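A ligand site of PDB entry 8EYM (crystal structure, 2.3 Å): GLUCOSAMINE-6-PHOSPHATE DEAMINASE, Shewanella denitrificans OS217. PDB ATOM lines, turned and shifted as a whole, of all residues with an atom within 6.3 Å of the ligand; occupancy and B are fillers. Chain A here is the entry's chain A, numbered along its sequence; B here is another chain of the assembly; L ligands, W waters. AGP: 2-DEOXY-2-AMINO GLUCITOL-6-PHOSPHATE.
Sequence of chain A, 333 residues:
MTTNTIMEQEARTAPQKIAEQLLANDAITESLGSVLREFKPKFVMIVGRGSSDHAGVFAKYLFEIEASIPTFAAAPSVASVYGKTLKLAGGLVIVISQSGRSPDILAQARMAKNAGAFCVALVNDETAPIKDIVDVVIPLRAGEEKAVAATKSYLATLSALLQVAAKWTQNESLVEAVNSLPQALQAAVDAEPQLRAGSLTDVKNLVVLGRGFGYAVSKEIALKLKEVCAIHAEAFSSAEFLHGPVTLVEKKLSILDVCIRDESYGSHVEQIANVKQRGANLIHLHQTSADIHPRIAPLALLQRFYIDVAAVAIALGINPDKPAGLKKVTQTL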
ATOM      1  N   GLY A  48      18.931 -13.881 -15.697  1.00  0.00           N
ATOM      2  CA  GLY A  48      17.940 -14.840 -16.147  1.00  0.00           C
ATOM      3  C   GLY A  48      18.615 -15.965 -16.899  1.00  0.00           C
ATOM      4  O   GLY A  48      19.800 -15.891 -17.249  1.00  0.00           O
ATOM      5  N   ARG A  49      17.837 -17.015 -17.153  1.00  0.00           N
ATOM      6  CA  ARG A  49      18.266 -18.195 -17.891  1.00  0.00           C
ATOM      7  C   ARG A  49      17.341 -18.430 -19.074  1.00  0.00           C
ATOM      8  O   ARG A  49      16.198 -17.949 -19.100  1.00  0.00           O
ATOM      9  CB  ARG A  49      18.254 -19.428 -16.990  1.00  0.00           C
ATOM     10  CG  ARG A  49      19.305 -19.372 -15.879  1.00  0.00           C
ATOM     11  CD  ARG A  49      20.638 -19.885 -16.403  1.00  0.00           C
ATOM     12  NE  ARG A  49      21.629 -20.022 -15.345  1.00  0.00           N
ATOM     13  CZ  ARG A  49      22.941 -19.859 -15.505  1.00  0.00           C
ATOM     14  NH1 ARG A  49      23.443 -19.566 -16.706  1.00  0.00           N
ATOM     15  NH2 ARG A  49      23.754 -20.009 -14.452  1.00  0.00           N
ATOM     16  N   GLY A  50      17.848 -19.187 -20.062  1.00  0.00           N
ATOM     17  CA  GLY A  50      17.041 -19.629 -21.198  1.00  0.00           C
ATOM     18  C   GLY A  50      16.358 -18.490 -21.927  1.00  0.00           C
ATOM     19  O   GLY A  50      16.996 -17.489 -22.298  1.00  0.00           O
ATOM     20  N   SER A  51      15.037 -18.615 -22.128  1.00  0.00           N
ATOM     21  CA  SER A  51      14.302 -17.569 -22.856  1.00  0.00           C
ATOM     22  C   SER A  51      14.404 -16.219 -22.159  1.00  0.00           C
ATOM     23  O   SER A  51      14.373 -15.174 -22.823  1.00  0.00           O
ATOM     24  CB  SER A  51      12.827 -17.959 -23.030  1.00  0.00           C
ATOM     25  OG  SER A  51      12.629 -18.856 -24.127  1.00  0.00           O
ATOM     26  N   SER A  52      14.525 -16.218 -20.828  1.00  0.00           N
ATOM     27  CA  SER A  52      14.685 -14.966 -20.090  1.00  0.00           C
ATOM     28  C   SER A  52      16.040 -14.324 -20.365  1.00  0.00           C
ATOM     29  O   SER A  52      16.144 -13.095 -20.460  1.00  0.00           O
ATOM     30  CB  SER A  52      14.493 -15.220 -18.605  1.00  0.00           C
ATOM     31  OG  SER A  52      13.166 -15.633 -18.364  1.00  0.00           O
ATOM     32  N   ASP A  53      17.097 -15.139 -20.499  1.00  0.00           N
ATOM     33  CA  ASP A  53      18.403 -14.615 -20.855  1.00  0.00           C
ATOM     34  C   ASP A  53      18.405 -14.004 -22.256  1.00  0.00           C
ATOM     35  O   ASP A  53      19.043 -12.974 -22.487  1.00  0.00           O
ATOM     36  CB  ASP A  53      19.472 -15.712 -20.771  1.00  0.00           C
ATOM     37  CG  ASP A  53      20.841 -15.251 -21.294  1.00  0.00           C
ATOM     38  OD1 ASP A  53      21.210 -15.634 -22.429  1.00  0.00           O
ATOM     39  OD2 ASP A  53      21.537 -14.494 -20.602  1.00  0.00           O
ATOM     40  N   ILE A  96      14.873 -11.459 -14.705  1.00  0.00           N
ATOM     41  CA  ILE A  96      13.837 -11.958 -15.600  1.00  0.00           C
ATOM     42  C   ILE A  96      13.649 -13.443 -15.312  1.00  0.00           C
ATOM     43  O   ILE A  96      14.589 -14.232 -15.417  1.00  0.00           O
ATOM     44  CB  ILE A  96      14.184 -11.673 -17.068  1.00  0.00           C
ATOM     45  CG1 ILE A  96      14.367 -10.170 -17.258  1.00  0.00           C
ATOM     46  CG2 ILE A  96      13.092 -12.187 -17.989  1.00  0.00           C
ATOM     47  CD1 ILE A  96      14.760  -9.753 -18.640  1.00  0.00           C
ATOM     48  N   SER A  97      12.423 -13.826 -14.958  1.00  0.00           N
ATOM     49  CA  SER A  97      12.099 -15.212 -14.664  1.00  0.00           C
ATOM     50  C   SER A  97      10.599 -15.397 -14.777  1.00  0.00           C
ATOM     51  O   SER A  97       9.839 -14.743 -14.063  1.00  0.00           O
ATOM     52  CB  SER A  97      12.535 -15.596 -13.256  1.00  0.00           C
ATOM     53  OG  SER A  97      12.412 -16.997 -13.107  1.00  0.00           O
ATOM     54  N   GLN A  98      10.193 -16.294 -15.673  1.00  0.00           N
ATOM     55  CA  GLN A  98       8.788 -16.646 -15.806  1.00  0.00           C
ATOM     56  C   GLN A  98       8.265 -17.220 -14.486  1.00  0.00           C
ATOM     57  O   GLN A  98       7.344 -16.685 -13.876  1.00  0.00           O
ATOM     58  CB  GLN A  98       8.602 -17.560 -17.025  1.00  0.00           C
ATOM     59  CG  GLN A  98       7.162 -17.787 -17.458  1.00  0.00           C
ATOM     60  CD  GLN A  98       6.474 -18.895 -16.686  1.00  0.00           C
ATOM     61  OE1 GLN A  98       5.380 -18.713 -16.148  1.00  0.00           O
ATOM     62  NE2 GLN A  98       7.088 -20.073 -16.667  1.00  0.00           N
ATOM     63  N   SER A  99       8.912 -18.280 -13.994  1.00  0.00           N
ATOM     64  CA  SER A  99       8.449 -18.889 -12.745  1.00  0.00           C
ATOM     65  C   SER A  99       8.711 -17.991 -11.553  1.00  0.00           C
ATOM     66  O   SER A  99       7.837 -17.810 -10.688  1.00  0.00           O
ATOM     67  CB  SER A  99       9.144 -20.241 -12.558  1.00  0.00           C
ATOM     68  OG  SER A  99      10.550 -20.103 -12.613  1.00  0.00           O
ATOM     69  N   GLY A 100       9.914 -17.414 -11.477  1.00  0.00           N
ATOM     70  CA  GLY A 100      10.306 -16.524 -10.393  1.00  0.00           C
ATOM     71  C   GLY A 100      10.582 -17.179  -9.058  1.00  0.00           C
ATOM     72  O   GLY A 100      10.618 -16.470  -8.047  1.00  0.00           O
ATOM     73  N   SER A 102      13.061 -20.150  -8.780  1.00  0.00           N
ATOM     74  CA  SER A 102      14.239 -21.010  -8.748  1.00  0.00           C
ATOM     75  C   SER A 102      15.256 -20.429  -7.769  1.00  0.00           C
ATOM     76  O   SER A 102      15.370 -19.209  -7.627  1.00  0.00           O
ATOM     77  CB  SER A 102      14.850 -21.194 -10.140  1.00  0.00           C
ATOM     78  OG  SER A 102      15.758 -20.153 -10.443  1.00  0.00           O
ATOM     79  N   ILE A 105      18.104 -18.186  -9.104  1.00  0.00           N
ATOM     80  CA  ILE A 105      17.620 -16.842  -9.402  1.00  0.00           C
ATOM     81  C   ILE A 105      17.480 -16.018  -8.136  1.00  0.00           C
ATOM     82  O   ILE A 105      17.895 -14.855  -8.089  1.00  0.00           O
ATOM     83  CB  ILE A 105      16.320 -16.903 -10.218  1.00  0.00           C
ATOM     84  CG1 ILE A 105      16.658 -17.230 -11.673  1.00  0.00           C
ATOM     85  CG2 ILE A 105      15.557 -15.614 -10.123  1.00  0.00           C
ATOM     86  CD1 ILE A 105      17.658 -16.282 -12.257  1.00  0.00           C
ATOM     87  N   ALA A 147       2.920 -25.138 -21.841  1.00  0.00           N
ATOM     88  CA  ALA A 147       3.835 -25.674 -22.833  1.00  0.00           C
ATOM     89  C   ALA A 147       5.257 -25.683 -22.270  1.00  0.00           C
ATOM     90  O   ALA A 147       5.616 -24.882 -21.410  1.00  0.00           O
ATOM     91  CB  ALA A 147       3.779 -24.830 -24.103  1.00  0.00           C
ATOM     92  N   VAL A 148       6.046 -26.653 -22.722  1.00  0.00           N
ATOM     93  CA  VAL A 148       7.463 -26.694 -22.387  1.00  0.00           C
ATOM     94  C   VAL A 148       8.178 -25.467 -22.943  1.00  0.00           C
ATOM     95  O   VAL A 148       8.997 -24.830 -22.271  1.00  0.00           O
ATOM     96  CB  VAL A 148       8.102 -28.014 -22.878  1.00  0.00           C
ATOM     97  CG1 VAL A 148       9.612 -27.900 -22.931  1.00  0.00           C
ATOM     98  CG2 VAL A 148       7.692 -29.149 -21.970  1.00  0.00           C
ATOM     99  N   ALA A 149       7.905 -25.133 -24.203  1.00  0.00           N
ATOM    100  CA  ALA A 149       8.475 -23.965 -24.866  1.00  0.00           C
ATOM    101  C   ALA A 149       7.764 -22.687 -24.429  1.00  0.00           C
ATOM    102  O   ALA A 149       6.550 -22.567 -24.618  1.00  0.00           O
ATOM    103  CB  ALA A 149       8.345 -24.110 -26.372  1.00  0.00           C
ATOM    104  N   ALA A 150       8.520 -21.723 -23.900  1.00  0.00           N
ATOM    105  CA  ALA A 150       7.947 -20.412 -23.642  1.00  0.00           C
ATOM    106  C   ALA A 150       7.597 -19.737 -24.967  1.00  0.00           C
ATOM    107  O   ALA A 150       8.347 -19.804 -25.950  1.00  0.00           O
ATOM    108  CB  ALA A 150       8.922 -19.526 -22.862  1.00  0.00           C
ATOM    109  N   THR A 151       6.419 -19.105 -25.013  1.00  0.00           N
ATOM    110  CA  THR A 151       6.040 -18.293 -26.149  1.00  0.00           C
ATOM    111  C   THR A 151       5.476 -16.969 -25.653  1.00  0.00           C
ATOM    112  O   THR A 151       6.139 -15.927 -25.744  1.00  0.00           O
ATOM    113  CB  THR A 151       5.035 -19.007 -27.096  1.00  0.00           C
ATOM    114  OG1 THR A 151       3.790 -19.270 -26.410  1.00  0.00           O
ATOM    115  CG2 THR A 151       5.608 -20.320 -27.618  1.00  0.00           C
ATOM    116  N   SER A 153       5.026 -15.939 -22.625  1.00  0.00           N
ATOM    117  CA  SER A 153       5.783 -15.345 -21.522  1.00  0.00           C
ATOM    118  C   SER A 153       7.025 -14.617 -22.004  1.00  0.00           C
ATOM    119  O   SER A 153       7.478 -13.657 -21.365  1.00  0.00           O
ATOM    120  CB  SER A 153       6.161 -16.422 -20.494  1.00  0.00           C
ATOM    121  OG  SER A 153       7.227 -17.218 -20.965  1.00  0.00           O
ATOM    122  N   GLU A 220      16.436 -16.437 -29.517  1.00  0.00           N
ATOM    123  CA  GLU A 220      15.203 -17.088 -29.093  1.00  0.00           C
ATOM    124  C   GLU A 220      14.674 -18.028 -30.170  1.00  0.00           C
ATOM    125  O   GLU A 220      14.140 -19.098 -29.844  1.00  0.00           O
ATOM    126  CB  GLU A 220      14.169 -16.035 -28.707  1.00  0.00           C
ATOM    127  CG  GLU A 220      12.749 -16.565 -28.542  1.00  0.00           C
ATOM    128  CD  GLU A 220      12.595 -17.499 -27.349  1.00  0.00           C
ATOM    129  OE1 GLU A 220      13.576 -17.676 -26.588  1.00  0.00           O
ATOM    130  OE2 GLU A 220      11.487 -18.045 -27.165  1.00  0.00           O
ATOM    131  N   LEU A 223      16.912 -21.088 -29.884  1.00  0.00           N
ATOM    132  CA  LEU A 223      16.556 -21.922 -28.700  1.00  0.00           C
ATOM    133  C   LEU A 223      15.296 -22.738 -28.987  1.00  0.00           C
ATOM    134  O   LEU A 223      15.273 -23.927 -28.648  1.00  0.00           O
ATOM    135  CB  LEU A 223      16.349 -21.004 -27.495  1.00  0.00           C
ATOM    136  CG  LEU A 223      15.901 -21.704 -26.217  1.00  0.00           C
ATOM    137  CD1 LEU A 223      16.817 -22.876 -25.889  1.00  0.00           C
ATOM    138  CD2 LEU A 223      15.853 -20.726 -25.045  1.00  0.00           C
ATOM    139  N   LYS A 224      14.313 -22.108 -29.623  1.00  0.00           N
ATOM    140  CA  LYS A 224      13.047 -22.797 -29.920  1.00  0.00           C
ATOM    141  C   LYS A 224      13.279 -23.920 -30.921  1.00  0.00           C
ATOM    142  O   LYS A 224      12.726 -24.955 -30.713  1.00  0.00           O
ATOM    143  CB  LYS A 224      11.976 -21.823 -30.435  1.00  0.00           C
ATOM    144  CG  LYS A 224      11.306 -20.937 -29.394  1.00  0.00           C
ATOM    145  CD  LYS A 224      10.637 -21.640 -28.274  1.00  0.00           C
ATOM    146  CE  LYS A 224      11.331 -21.450 -26.956  1.00  0.00           C
ATOM    147  NZ  LYS A 224      10.391 -21.327 -25.826  1.00  0.00           N
ATOM    148  N   GLU A 227      14.617 -26.651 -28.902  1.00  0.00           N
ATOM    149  CA  GLU A 227      13.750 -27.142 -27.842  1.00  0.00           C
ATOM    150  C   GLU A 227      12.592 -27.961 -28.391  1.00  0.00           C
ATOM    151  O   GLU A 227      12.252 -29.010 -27.829  1.00  0.00           O
ATOM    152  CB  GLU A 227      13.273 -25.980 -26.984  1.00  0.00           C
ATOM    153  CG  GLU A 227      12.781 -26.411 -25.623  1.00  0.00           C
ATOM    154  CD  GLU A 227      12.424 -25.239 -24.738  1.00  0.00           C
ATOM    155  OE1 GLU A 227      12.513 -24.100 -25.234  1.00  0.00           O
ATOM    156  OE2 GLU A 227      12.101 -25.460 -23.547  1.00  0.00           O
ATOM    157  N   GLU B 240      23.637 -23.570 -18.215  1.00  0.00           N
ATOM    158  CA  GLU B 240      22.682 -23.102 -19.208  1.00  0.00           C
ATOM    159  C   GLU B 240      22.130 -24.226 -20.087  1.00  0.00           C
ATOM    160  O   GLU B 240      20.984 -24.162 -20.527  1.00  0.00           O
ATOM    161  CB  GLU B 240      23.334 -22.005 -20.047  1.00  0.00           C
ATOM    162  CG  GLU B 240      22.423 -21.362 -21.061  1.00  0.00           C
ATOM    163  CD  GLU B 240      21.487 -20.351 -20.404  1.00  0.00           C
ATOM    164  OE1 GLU B 240      21.986 -19.464 -19.648  1.00  0.00           O
ATOM    165  OE2 GLU B 240      20.264 -20.457 -20.644  1.00  0.00           O
ATOM    166  N   LEU B 242      20.926 -27.060 -19.660  1.00  0.00           N
ATOM    167  CA  LEU B 242      19.701 -27.762 -19.261  1.00  0.00           C
ATOM    168  C   LEU B 242      18.435 -26.987 -19.591  1.00  0.00           C
ATOM    169  O   LEU B 242      17.360 -27.605 -19.665  1.00  0.00           O
ATOM    170  CB  LEU B 242      19.746 -28.148 -17.777  1.00  0.00           C
ATOM    171  CG  LEU B 242      20.779 -29.217 -17.402  1.00  0.00           C
ATOM    172  CD1 LEU B 242      20.815 -29.443 -15.892  1.00  0.00           C
ATOM    173  CD2 LEU B 242      20.553 -30.527 -18.139  1.00  0.00           C
ATOM    174  N   HIS B 243      18.523 -25.676 -19.823  1.00  0.00           N
ATOM    175  CA  HIS B 243      17.316 -24.867 -20.022  1.00  0.00           C
ATOM    176  C   HIS B 243      16.892 -24.856 -21.490  1.00  0.00           C
ATOM    177  O   HIS B 243      16.728 -23.797 -22.105  1.00  0.00           O
ATOM    178  CB  HIS B 243      17.523 -23.446 -19.510  1.00  0.00           C
ATOM    179  CG  HIS B 243      17.823 -23.366 -18.052  1.00  0.00           C
ATOM    180  ND1 HIS B 243      16.853 -23.156 -17.088  1.00  0.00           N
ATOM    181  CD2 HIS B 243      18.997 -23.461 -17.365  1.00  0.00           C
ATOM    182  CE1 HIS B 243      17.414 -23.118 -15.892  1.00  0.00           C
ATOM    183  NE2 HIS B 243      18.712 -23.300 -16.035  1.00  0.00           N
ATOM    184  N   GLY B 244      16.727 -26.043 -22.082  1.00  0.00           N
ATOM    185  CA  GLY B 244      16.305 -26.155 -23.459  1.00  0.00           C
ATOM    186  C   GLY B 244      17.248 -26.911 -24.374  1.00  0.00           C
ATOM    187  O   GLY B 244      16.848 -27.890 -25.030  1.00  0.00           O
ATOM    188  N   PRO B 245      18.511 -26.465 -24.477  1.00  0.00           N
ATOM    189  CA  PRO B 245      19.424 -27.101 -25.449  1.00  0.00           C
ATOM    190  C   PRO B 245      19.665 -28.584 -25.204  1.00  0.00           C
ATOM    191  O   PRO B 245      19.975 -29.323 -26.145  1.00  0.00           O
ATOM    192  CB  PRO B 245      20.707 -26.281 -25.313  1.00  0.00           C
ATOM    193  CG  PRO B 245      20.224 -24.938 -24.868  1.00  0.00           C
ATOM    194  CD  PRO B 245      19.063 -25.209 -23.955  1.00  0.00           C
HETATM  195  C1  AGP L   1      12.325 -21.643 -22.782  1.00  0.00           C
HETATM  196  O1  AGP L   1      11.327 -22.069 -23.723  1.00  0.00           O
HETATM  197  C2  AGP L   1      12.762 -22.804 -21.886  1.00  0.00           C
HETATM  198  N2  AGP L   1      11.630 -23.453 -21.225  1.00  0.00           N
HETATM  199  C3  AGP L   1      13.768 -22.375 -20.815  1.00  0.00           C
HETATM  200  O3  AGP L   1      14.980 -21.987 -21.462  1.00  0.00           O
HETATM  201  C4  AGP L   1      13.291 -21.255 -19.879  1.00  0.00           C
HETATM  202  O4  AGP L   1      13.346 -19.964 -20.506  1.00  0.00           O
HETATM  203  C5  AGP L   1      14.145 -21.197 -18.628  1.00  0.00           C
HETATM  204  O5  AGP L   1      14.747 -22.452 -18.330  1.00  0.00           O
HETATM  205  C6  AGP L   1      13.286 -20.884 -17.438  1.00  0.00           C
HETATM  206  O6  AGP L   1      13.431 -19.504 -17.195  1.00  0.00           O
HETATM  207  P   AGP L   1      12.377 -18.791 -16.226  1.00  0.00           P
HETATM  208  O1P AGP L   1      13.158 -18.538 -14.950  1.00  0.00           O
HETATM  209  O2P AGP L   1      11.270 -19.810 -16.089  1.00  0.00           O
HETATM  210  O3P AGP L   1      12.044 -17.554 -17.029  1.00  0.00           O
HETATM  211  O   HOH W   1      13.707 -25.455 -19.805  1.00  0.00           O
HETATM  212  O   HOH W   2      15.304 -16.785 -15.716  1.00  0.00           O
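The side-chain amino group (NZ) of Lys 224 is in salt-bridge range of the side-chain carboxylate (OE2) of Glu 220. The side-chain hydroxyl of Ser 51 lies within hydrogen-bond range of the side-chain carboxylate of Glu 220 (2.9 Å). N of Gly 50 lies within hydrogen-bond range of OE2 of Glu 240 of chain B, at 2.8 Å. O of Ala 150 sits at hydrogen-bond distance from NZ of Lys 224 (2.6 Å). The side-chain carboxylate of Glu 240 of chain B lies within salt-bridge range of the guanidinium group of Arg 49, 3.3 Å away. The side-chain amino group (NZ) of Lys 224 lies within salt-bridge range of the side-chain carboxylate (OE1) of Glu 227. The side-chain hydroxyl of Ser 97 sits at hydrogen-bond distance from the backbone NH of Gly 100, at 3.0 Å.
Arg 49 touches the ligand. Gly 50 touches the ligand (CA to O3, 3.1 Å). Ser 99 touches the ligand. Ala 149 touches the ligand (CA to O1, 3.6 Å). Leu 223 touches the ligand. Hydrophobic or aromatic side chains that line the ligand: Ala 150, Leu 223 and His 243 of chain B. 14 residues have an atom within 4 Å of the ligand: Arg 49, Gly 50, Ser 51, Ser 52, Ser 97, Gln 98, Ser 99, Val 148, Ala 149, Ala 150, Leu 223, Lys 224, Glu 227 and His 243 of chain B. The nearest printed residue that does not touch the ligand is Gly 244 of chain B (4.5 Å).
NZ of Lys 224 sits at hydrogen-bond distance from O1 of the ligand (2.4 Å). O of His 243 of chain B sits at hydrogen-bond distance from O3 of the ligand, 2.6 Å away. The backbone carbonyl oxygen (O) of Val 148 is in hydrogen-bond range of a nitrogen (N2) of the ligand (3.2 Å). The backbone NH (N) of Ser 51 lies within hydrogen-bond range of an oxygen (O4) of the ligand (2.7 Å). OE2 of Glu 227 lies within salt-bridge range of N2 of the ligand. OG of Ser 51 sits close to O1 of the ligand, at 3.5 Å. The backbone NH (N) of Ala 150 sits at hydrogen-bond distance from an oxygen (O1) of the ligand (2.8 Å). O1P of the ligand lies within hydrogen-bond range of OG of Ser 97 (2.5 Å). ND1 of His 243 of chain B is in hydrogen-bond range of O5 of the ligand (2.5 Å). N of Gln 98 sits at hydrogen-bond distance from O3P of the ligand (2.6 Å). An oxygen (O3P) of the ligand lies within hydrogen-bond range of the side-chain hydroxyl (OG) of Ser 52 (2.6 Å).
Water W2 lies within hydrogen-bond range of O of Ile 96 (2.7 Å), O1P of the ligand (2.9 Å) and N of Arg 49 (2.9 Å).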
